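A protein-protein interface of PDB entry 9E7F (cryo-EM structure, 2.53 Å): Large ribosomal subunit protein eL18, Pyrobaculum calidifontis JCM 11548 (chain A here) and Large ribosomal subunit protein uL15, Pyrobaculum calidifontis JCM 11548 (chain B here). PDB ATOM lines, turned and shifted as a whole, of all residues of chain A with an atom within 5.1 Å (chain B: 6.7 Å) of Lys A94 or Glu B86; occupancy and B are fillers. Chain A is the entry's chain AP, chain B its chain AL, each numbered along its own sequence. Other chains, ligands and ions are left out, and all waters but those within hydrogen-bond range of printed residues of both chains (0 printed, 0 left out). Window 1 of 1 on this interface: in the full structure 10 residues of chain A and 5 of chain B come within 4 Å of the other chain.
The side-chain carboxylate (OE2) of Glu B86 sits close to the backbone NH (N) of Glu A75.
OE2 of Glu B86 lies within salt-bridge range of NZ of Lys A94.
The side-chain carboxylate (OE2) of Glu B90 lies within salt-bridge range of the side-chain amino group (NZ) of Lys A90 (2.6 Å).
The backbone carbonyl oxygen (O) of Gly A74 sits close to the side-chain carboxylate (OE2) of Glu B86 (2.9 Å).
The side-chain carboxylate of Glu B86 lies within salt-bridge range of the guanidinium group of Arg B83, 3.2 Å away.
O of Gly A74 sits at hydrogen-bond distance from NZ of Lys A94 (2.7 Å).
Glu A75 touches Ala B85 (OE1 to C, 3.9 Å).
Printed residues of chain B within 4 Å of Gly A74: Glu B86.
Of the printed residues of chain B, Glu A75 touches Ala B85 and Glu B86.
Printed residues of chain B within 4 Å of Lys A90: Glu B90 (2.6 Å).
Lys A94 touches one residue of chain B.
Glu B86 touches just these residues of chain A: Gly A74 (2.9 Å), Glu A75 (2.8 Å) and Lys A94 (3.6 Å).
Printed residues of chain A within 4 Å of Glu B90: Lys A90 (2.6 Å).
The nearest printed residue of chain B that does not touch Glu A75 is Lys B89 (4.2 Å).
Of the 15 printed residues of chain A, 4 touch a printed residue of chain B.
Printed residues of chain B that touch a printed residue of chain A: Ala B85, Glu B86 and Glu B90.
Among the printed residues, Asp or Glu carboxylates within 4 Å of a Lys or Arg side-chain nitrogen of the other chain: Lys A90 with Glu B90 (2.6 Å) and Lys A94 with Glu B86 (3.6 Å).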
ATOM      1  N   VAL A  51      -5.708  22.999  18.466  1.00  0.00           N
ATOM      2  CA  VAL A  51      -6.433  24.127  17.891  1.00  0.00           C
ATOM      3  C   VAL A  51      -7.841  24.221  18.454  1.00  0.00           C
ATOM      4  O   VAL A  51      -8.458  25.291  18.420  1.00  0.00           O
ATOM      5  CB  VAL A  51      -6.449  24.020  16.359  1.00  0.00           C
ATOM      6  CG1 VAL A  51      -5.055  24.198  15.815  1.00  0.00           C
ATOM      7  CG2 VAL A  51      -7.022  22.688  15.938  1.00  0.00           C
ATOM      8  N   GLY A  72      -2.879  19.778  16.170  1.00  0.00           N
ATOM      9  CA  GLY A  72      -4.162  19.865  15.506  1.00  0.00           C
ATOM     10  C   GLY A  72      -5.215  18.965  16.108  1.00  0.00           C
ATOM     11  O   GLY A  72      -5.320  17.794  15.743  1.00  0.00           O
ATOM     12  N   GLY A  73      -6.023  19.505  17.002  1.00  0.00           N
ATOM     13  CA  GLY A  73      -7.067  18.733  17.643  1.00  0.00           C
ATOM     14  C   GLY A  73      -8.297  19.591  17.826  1.00  0.00           C
ATOM     15  O   GLY A  73      -8.209  20.797  18.059  1.00  0.00           O
ATOM     16  N   GLY A  74      -9.450  18.957  17.714  1.00  0.00           N
ATOM     17  CA  GLY A  74     -10.662  19.734  17.687  1.00  0.00           C
ATOM     18  C   GLY A  74     -10.778  20.485  16.370  1.00  0.00           C
ATOM     19  O   GLY A  74     -10.011  20.292  15.430  1.00  0.00           O
ATOM     20  N   GLU A  75     -11.785  21.346  16.313  1.00  0.00           N
ATOM     21  CA  GLU A  75     -12.051  22.151  15.134  1.00  0.00           C
ATOM     22  C   GLU A  75     -11.996  23.621  15.509  1.00  0.00           C
ATOM     23  O   GLU A  75     -12.542  24.028  16.538  1.00  0.00           O
ATOM     24  CB  GLU A  75     -13.415  21.813  14.525  1.00  0.00           C
ATOM     25  CG  GLU A  75     -13.357  20.792  13.401  1.00  0.00           C
ATOM     26  CD  GLU A  75     -14.574  19.889  13.375  1.00  0.00           C
ATOM     27  OE1 GLU A  75     -14.403  18.655  13.425  1.00  0.00           O
ATOM     28  OE2 GLU A  75     -15.704  20.415  13.299  1.00  0.00           O
ATOM     29  N   LEU A  76     -11.330  24.412  14.677  1.00  0.00           N
ATOM     30  CA  LEU A  76     -11.188  25.840  14.906  1.00  0.00           C
ATOM     31  C   LEU A  76     -12.181  26.578  14.019  1.00  0.00           C
ATOM     32  O   LEU A  76     -12.119  26.473  12.791  1.00  0.00           O
ATOM     33  CB  LEU A  76      -9.759  26.300  14.621  1.00  0.00           C
ATOM     34  CG  LEU A  76      -9.344  27.608  15.296  1.00  0.00           C
ATOM     35  CD1 LEU A  76      -9.827  27.633  16.734  1.00  0.00           C
ATOM     36  CD2 LEU A  76      -7.844  27.796  15.240  1.00  0.00           C
ATOM     37  N   LYS A  90      -1.522  19.631  10.421  1.00  0.00           N
ATOM     38  CA  LYS A  90      -2.962  19.718  10.635  1.00  0.00           C
ATOM     39  C   LYS A  90      -3.340  21.002  11.363  1.00  0.00           C
ATOM     40  O   LYS A  90      -4.388  21.591  11.084  1.00  0.00           O
ATOM     41  CB  LYS A  90      -3.448  18.497  11.413  1.00  0.00           C
ATOM     42  CG  LYS A  90      -4.910  18.544  11.799  1.00  0.00           C
ATOM     43  CD  LYS A  90      -5.320  17.279  12.517  1.00  0.00           C
ATOM     44  CE  LYS A  90      -6.732  16.881  12.154  1.00  0.00           C
ATOM     45  NZ  LYS A  90      -6.785  15.577  11.439  1.00  0.00           N
ATOM     46  N   ALA A  91      -2.509  21.444  12.309  1.00  0.00           N
ATOM     47  CA  ALA A  91      -2.790  22.687  13.019  1.00  0.00           C
ATOM     48  C   ALA A  91      -2.680  23.896  12.099  1.00  0.00           C
ATOM     49  O   ALA A  91      -3.491  24.824  12.184  1.00  0.00           O
ATOM     50  CB  ALA A  91      -1.844  22.837  14.205  1.00  0.00           C
ATOM     51  N   TRP A  92      -1.669  23.909  11.227  1.00  0.00           N
ATOM     52  CA  TRP A  92      -1.506  25.005  10.276  1.00  0.00           C
ATOM     53  C   TRP A  92      -2.685  25.062   9.313  1.00  0.00           C
ATOM     54  O   TRP A  92      -3.170  26.147   8.980  1.00  0.00           O
ATOM     55  CB  TRP A  92      -0.180  24.830   9.522  1.00  0.00           C
ATOM     56  CG  TRP A  92       0.361  26.013   8.708  1.00  0.00           C
ATOM     57  CD1 TRP A  92      -0.341  27.050   8.160  1.00  0.00           C
ATOM     58  CD2 TRP A  92       1.728  26.226   8.330  1.00  0.00           C
ATOM     59  NE1 TRP A  92       0.498  27.895   7.484  1.00  0.00           N
ATOM     60  CE2 TRP A  92       1.776  27.413   7.572  1.00  0.00           C
ATOM     61  CE3 TRP A  92       2.920  25.531   8.567  1.00  0.00           C
ATOM     62  CZ2 TRP A  92       2.964  27.921   7.051  1.00  0.00           C
ATOM     63  CZ3 TRP A  92       4.099  26.036   8.045  1.00  0.00           C
ATOM     64  CH2 TRP A  92       4.111  27.220   7.298  1.00  0.00           C
ATOM     65  N   LYS A  93      -3.147  23.905   8.838  1.00  0.00           N
ATOM     66  CA  LYS A  93      -4.272  23.895   7.911  1.00  0.00           C
ATOM     67  C   LYS A  93      -5.554  24.358   8.593  1.00  0.00           C
ATOM     68  O   LYS A  93      -6.325  25.130   8.016  1.00  0.00           O
ATOM     69  CB  LYS A  93      -4.444  22.497   7.318  1.00  0.00           C
ATOM     70  CG  LYS A  93      -5.627  22.357   6.391  1.00  0.00           C
ATOM     71  CD  LYS A  93      -6.318  21.020   6.566  1.00  0.00           C
ATOM     72  CE  LYS A  93      -5.320  19.884   6.662  1.00  0.00           C
ATOM     73  NZ  LYS A  93      -5.985  18.552   6.733  1.00  0.00           N
ATOM     74  N   LYS A  94      -5.790  23.915   9.826  1.00  0.00           N
ATOM     75  CA  LYS A  94      -7.010  24.304  10.519  1.00  0.00           C
ATOM     76  C   LYS A  94      -7.003  25.779  10.895  1.00  0.00           C
ATOM     77  O   LYS A  94      -8.063  26.412  10.921  1.00  0.00           O
ATOM     78  CB  LYS A  94      -7.214  23.438  11.759  1.00  0.00           C
ATOM     79  CG  LYS A  94      -7.750  22.059  11.441  1.00  0.00           C
ATOM     80  CD  LYS A  94      -7.949  21.235  12.686  1.00  0.00           C
ATOM     81  CE  LYS A  94      -8.430  19.844  12.339  1.00  0.00           C
ATOM     82  NZ  LYS A  94      -8.618  19.021  13.558  1.00  0.00           N
ATOM     83  N   VAL A  95      -5.832  26.338  11.204  1.00  0.00           N
ATOM     84  CA  VAL A  95      -5.750  27.760  11.523  1.00  0.00           C
ATOM     85  C   VAL A  95      -5.967  28.603  10.277  1.00  0.00           C
ATOM     86  O   VAL A  95      -6.647  29.633  10.319  1.00  0.00           O
ATOM     87  CB  VAL A  95      -4.405  28.084  12.190  1.00  0.00           C
ATOM     88  CG1 VAL A  95      -4.023  29.521  11.911  1.00  0.00           C
ATOM     89  CG2 VAL A  95      -4.483  27.833  13.680  1.00  0.00           C
ATOM     90  N   VAL A  96      -5.377  28.194   9.156  1.00  0.00           N
ATOM     91  CA  VAL A  96      -5.472  28.981   7.931  1.00  0.00           C
ATOM     92  C   VAL A  96      -6.893  28.958   7.387  1.00  0.00           C
ATOM     93  O   VAL A  96      -7.449  29.995   7.014  1.00  0.00           O
ATOM     94  CB  VAL A  96      -4.461  28.469   6.891  1.00  0.00           C
ATOM     95  CG1 VAL A  96      -4.814  28.994   5.521  1.00  0.00           C
ATOM     96  CG2 VAL A  96      -3.059  28.887   7.271  1.00  0.00           C
ATOM     97  N   GLU A  97      -7.506  27.775   7.342  1.00  0.00           N
ATOM     98  CA  GLU A  97      -8.840  27.649   6.772  1.00  0.00           C
ATOM     99  C   GLU A  97      -9.917  28.256   7.658  1.00  0.00           C
ATOM    100  O   GLU A  97     -11.031  28.480   7.176  1.00  0.00           O
ATOM    101  CB  GLU A  97      -9.154  26.181   6.487  1.00  0.00           C
ATOM    102  CG  GLU A  97      -8.806  25.773   5.063  1.00  0.00           C
ATOM    103  CD  GLU A  97      -8.152  24.410   4.978  1.00  0.00           C
ATOM    104  OE1 GLU A  97      -8.660  23.462   5.611  1.00  0.00           O
ATOM    105  OE2 GLU A  97      -7.124  24.288   4.285  1.00  0.00           O
ATOM    106  N   ALA A  98      -9.618  28.524   8.924  1.00  0.00           N
ATOM    107  CA  ALA A  98     -10.516  29.257   9.801  1.00  0.00           C
ATOM    108  C   ALA A  98     -10.378  30.763   9.648  1.00  0.00           C
ATOM    109  O   ALA A  98     -11.101  31.507  10.316  1.00  0.00           O
ATOM    110  CB  ALA A  98     -10.270  28.862  11.257  1.00  0.00           C
ATOM    111  N   VAL B  81     -19.725  11.642  18.599  1.00  0.00           N
ATOM    112  CA  VAL B  81     -20.183  12.349  17.406  1.00  0.00           C
ATOM    113  C   VAL B  81     -19.303  13.560  17.131  1.00  0.00           C
ATOM    114  O   VAL B  81     -19.062  13.917  15.972  1.00  0.00           O
ATOM    115  CB  VAL B  81     -21.666  12.735  17.547  1.00  0.00           C
ATOM    116  CG1 VAL B  81     -21.994  13.909  16.658  1.00  0.00           C
ATOM    117  CG2 VAL B  81     -22.543  11.553  17.199  1.00  0.00           C
ATOM    118  N   GLY B  82     -18.814  14.211  18.187  1.00  0.00           N
ATOM    119  CA  GLY B  82     -17.860  15.293  18.001  1.00  0.00           C
ATOM    120  C   GLY B  82     -16.580  14.831  17.329  1.00  0.00           C
ATOM    121  O   GLY B  82     -16.036  15.523  16.468  1.00  0.00           O
ATOM    122  N   ARG B  83     -16.086  13.654  17.712  1.00  0.00           N
ATOM    123  CA  ARG B  83     -14.986  13.041  16.978  1.00  0.00           C
ATOM    124  C   ARG B  83     -15.430  12.574  15.601  1.00  0.00           C
ATOM    125  O   ARG B  83     -14.649  12.622  14.647  1.00  0.00           O
ATOM    126  CB  ARG B  83     -14.419  11.868  17.772  1.00  0.00           C
ATOM    127  CG  ARG B  83     -13.331  11.099  17.052  1.00  0.00           C
ATOM    128  CD  ARG B  83     -11.994  11.797  17.160  1.00  0.00           C
ATOM    129  NE  ARG B  83     -11.020  11.233  16.236  1.00  0.00           N
ATOM    130  CZ  ARG B  83     -10.341  11.936  15.342  1.00  0.00           C
ATOM    131  NH1 ARG B  83     -10.469  13.249  15.254  1.00  0.00           N
ATOM    132  NH2 ARG B  83      -9.512  11.306  14.517  1.00  0.00           N
ATOM    133  N   LEU B  84     -16.672  12.108  15.483  1.00  0.00           N
ATOM    134  CA  LEU B  84     -17.179  11.660  14.196  1.00  0.00           C
ATOM    135  C   LEU B  84     -17.338  12.816  13.221  1.00  0.00           C
ATOM    136  O   LEU B  84     -17.295  12.605  12.005  1.00  0.00           O
ATOM    137  CB  LEU B  84     -18.509  10.941  14.385  1.00  0.00           C
ATOM    138  CG  LEU B  84     -19.232  10.532  13.107  1.00  0.00           C
ATOM    139  CD1 LEU B  84     -18.373   9.590  12.294  1.00  0.00           C
ATOM    140  CD2 LEU B  84     -20.562   9.897  13.445  1.00  0.00           C
ATOM    141  N   ALA B  85     -17.547  14.032  13.731  1.00  0.00           N
ATOM    142  CA  ALA B  85     -17.597  15.200  12.858  1.00  0.00           C
ATOM    143  C   ALA B  85     -16.259  15.423  12.170  1.00  0.00           C
ATOM    144  O   ALA B  85     -16.210  15.775  10.988  1.00  0.00           O
ATOM    145  CB  ALA B  85     -18.002  16.437  13.657  1.00  0.00           C
ATOM    146  N   GLU B  86     -15.161  15.217  12.896  1.00  0.00           N
ATOM    147  CA  GLU B  86     -13.839  15.354  12.300  1.00  0.00           C
ATOM    148  C   GLU B  86     -13.595  14.307  11.225  1.00  0.00           C
ATOM    149  O   GLU B  86     -12.976  14.598  10.197  1.00  0.00           O
ATOM    150  CB  GLU B  86     -12.771  15.251  13.382  1.00  0.00           C
ATOM    151  CG  GLU B  86     -12.993  16.185  14.529  1.00  0.00           C
ATOM    152  CD  GLU B  86     -11.779  17.029  14.799  1.00  0.00           C
ATOM    153  OE1 GLU B  86     -10.693  16.458  15.034  1.00  0.00           O
ATOM    154  OE2 GLU B  86     -11.910  18.265  14.739  1.00  0.00           O
ATOM    155  N   LEU B  87     -14.055  13.076  11.453  1.00  0.00           N
ATOM    156  CA  LEU B  87     -13.737  11.989  10.534  1.00  0.00           C
ATOM    157  C   LEU B  87     -14.428  12.169   9.190  1.00  0.00           C
ATOM    158  O   LEU B  87     -13.838  11.889   8.140  1.00  0.00           O
ATOM    159  CB  LEU B  87     -14.111  10.649  11.159  1.00  0.00           C
ATOM    160  CG  LEU B  87     -12.982  10.031  11.979  1.00  0.00           C
ATOM    161  CD1 LEU B  87     -13.450   8.773  12.670  1.00  0.00           C
ATOM    162  CD2 LEU B  87     -11.779   9.746  11.094  1.00  0.00           C
ATOM    163  N   VAL B  88     -15.678  12.630   9.197  1.00  0.00           N
ATOM    164  CA  VAL B  88     -16.404  12.810   7.943  1.00  0.00           C
ATOM    165  C   VAL B  88     -15.798  13.949   7.135  1.00  0.00           C
ATOM    166  O   VAL B  88     -15.732  13.887   5.901  1.00  0.00           O
ATOM    167  CB  VAL B  88     -17.902  13.036   8.218  1.00  0.00           C
ATOM    168  CG1 VAL B  88     -18.091  14.059   9.325  1.00  0.00           C
ATOM    169  CG2 VAL B  88     -18.613  13.472   6.947  1.00  0.00           C
ATOM    170  N   LYS B  89     -15.359  15.013   7.811  1.00  0.00           N
ATOM    171  CA  LYS B  89     -14.668  16.097   7.121  1.00  0.00           C
ATOM    172  C   LYS B  89     -13.358  15.614   6.519  1.00  0.00           C
ATOM    173  O   LYS B  89     -12.995  16.003   5.403  1.00  0.00           O
ATOM    174  CB  LYS B  89     -14.410  17.254   8.082  1.00  0.00           C
ATOM    175  CG  LYS B  89     -15.644  17.780   8.774  1.00  0.00           C
ATOM    176  CD  LYS B  89     -15.418  19.189   9.281  1.00  0.00           C
ATOM    177  CE  LYS B  89     -16.081  20.200   8.373  1.00  0.00           C
ATOM    178  NZ  LYS B  89     -17.439  19.752   7.965  1.00  0.00           N
ATOM    179  N   GLU B  90     -12.626  14.776   7.253  1.00  0.00           N
ATOM    180  CA  GLU B  90     -11.391  14.210   6.726  1.00  0.00           C
ATOM    181  C   GLU B  90     -11.663  13.305   5.532  1.00  0.00           C
ATOM    182  O   GLU B  90     -10.912  13.315   4.552  1.00  0.00           O
ATOM    183  CB  GLU B  90     -10.662  13.445   7.829  1.00  0.00           C
ATOM    184  CG  GLU B  90      -9.939  14.331   8.826  1.00  0.00           C
ATOM    185  CD  GLU B  90      -9.635  13.618  10.131  1.00  0.00           C
ATOM    186  OE1 GLU B  90     -10.012  12.436  10.267  1.00  0.00           O
ATOM    187  OE2 GLU B  90      -9.012  14.239  11.019  1.00  0.00           O
ATOM    188  N   LEU B  91     -12.733  12.509   5.602  1.00  0.00           N
ATOM    189  CA  LEU B  91     -13.083  11.627   4.493  1.00  0.00           C
ATOM    190  C   LEU B  91     -13.694  12.402   3.337  1.00  0.00           C
ATOM    191  O   LEU B  91     -13.572  11.992   2.177  1.00  0.00           O
ATOM    192  CB  LEU B  91     -14.047  10.544   4.964  1.00  0.00           C
ATOM    193  CG  LEU B  91     -13.437   9.404   5.772  1.00  0.00           C
ATOM    194  CD1 LEU B  91     -14.393   8.965   6.866  1.00  0.00           C
ATOM    195  CD2 LEU B  91     -13.089   8.246   4.859  1.00  0.00           C
ATOM    196  N   HIS B 121     -20.085  17.928  19.259  1.00  0.00           N
ATOM    197  CA  HIS B 121     -21.144  18.545  18.473  1.00  0.00           C
ATOM    198  C   HIS B 121     -21.140  17.980  17.062  1.00  0.00           C
ATOM    199  O   HIS B 121     -20.078  17.728  16.485  1.00  0.00           O
ATOM    200  CB  HIS B 121     -20.990  20.067  18.387  1.00  0.00           C
ATOM    201  CG  HIS B 121     -20.318  20.681  19.573  1.00  0.00           C
ATOM    202  ND1 HIS B 121     -18.950  20.701  19.726  1.00  0.00           N
ATOM    203  CD2 HIS B 121     -20.827  21.316  20.656  1.00  0.00           C
ATOM    204  CE1 HIS B 121     -18.644  21.311  20.856  1.00  0.00           C
ATOM    205  NE2 HIS B 121     -19.765  21.694  21.440  1.00  0.00           N
ATOM    206  N   MET B 122     -22.332  17.797  16.512  1.00  0.00           N
ATOM    207  CA  MET B 122     -22.509  17.507  15.098  1.00  0.00           C
ATOM    208  C   MET B 122     -23.061  18.757  14.427  1.00  0.00           C
ATOM    209  O   MET B 122     -24.007  19.372  14.928  1.00  0.00           O
ATOM    210  CB  MET B 122     -23.465  16.331  14.893  1.00  0.00           C
ATOM    211  CG  MET B 122     -23.606  15.870  13.456  1.00  0.00           C
ATOM    212  SD  MET B 122     -22.529  14.486  13.046  1.00  0.00           S
ATOM    213  CE  MET B 122     -20.989  15.327  12.716  1.00  0.00           C
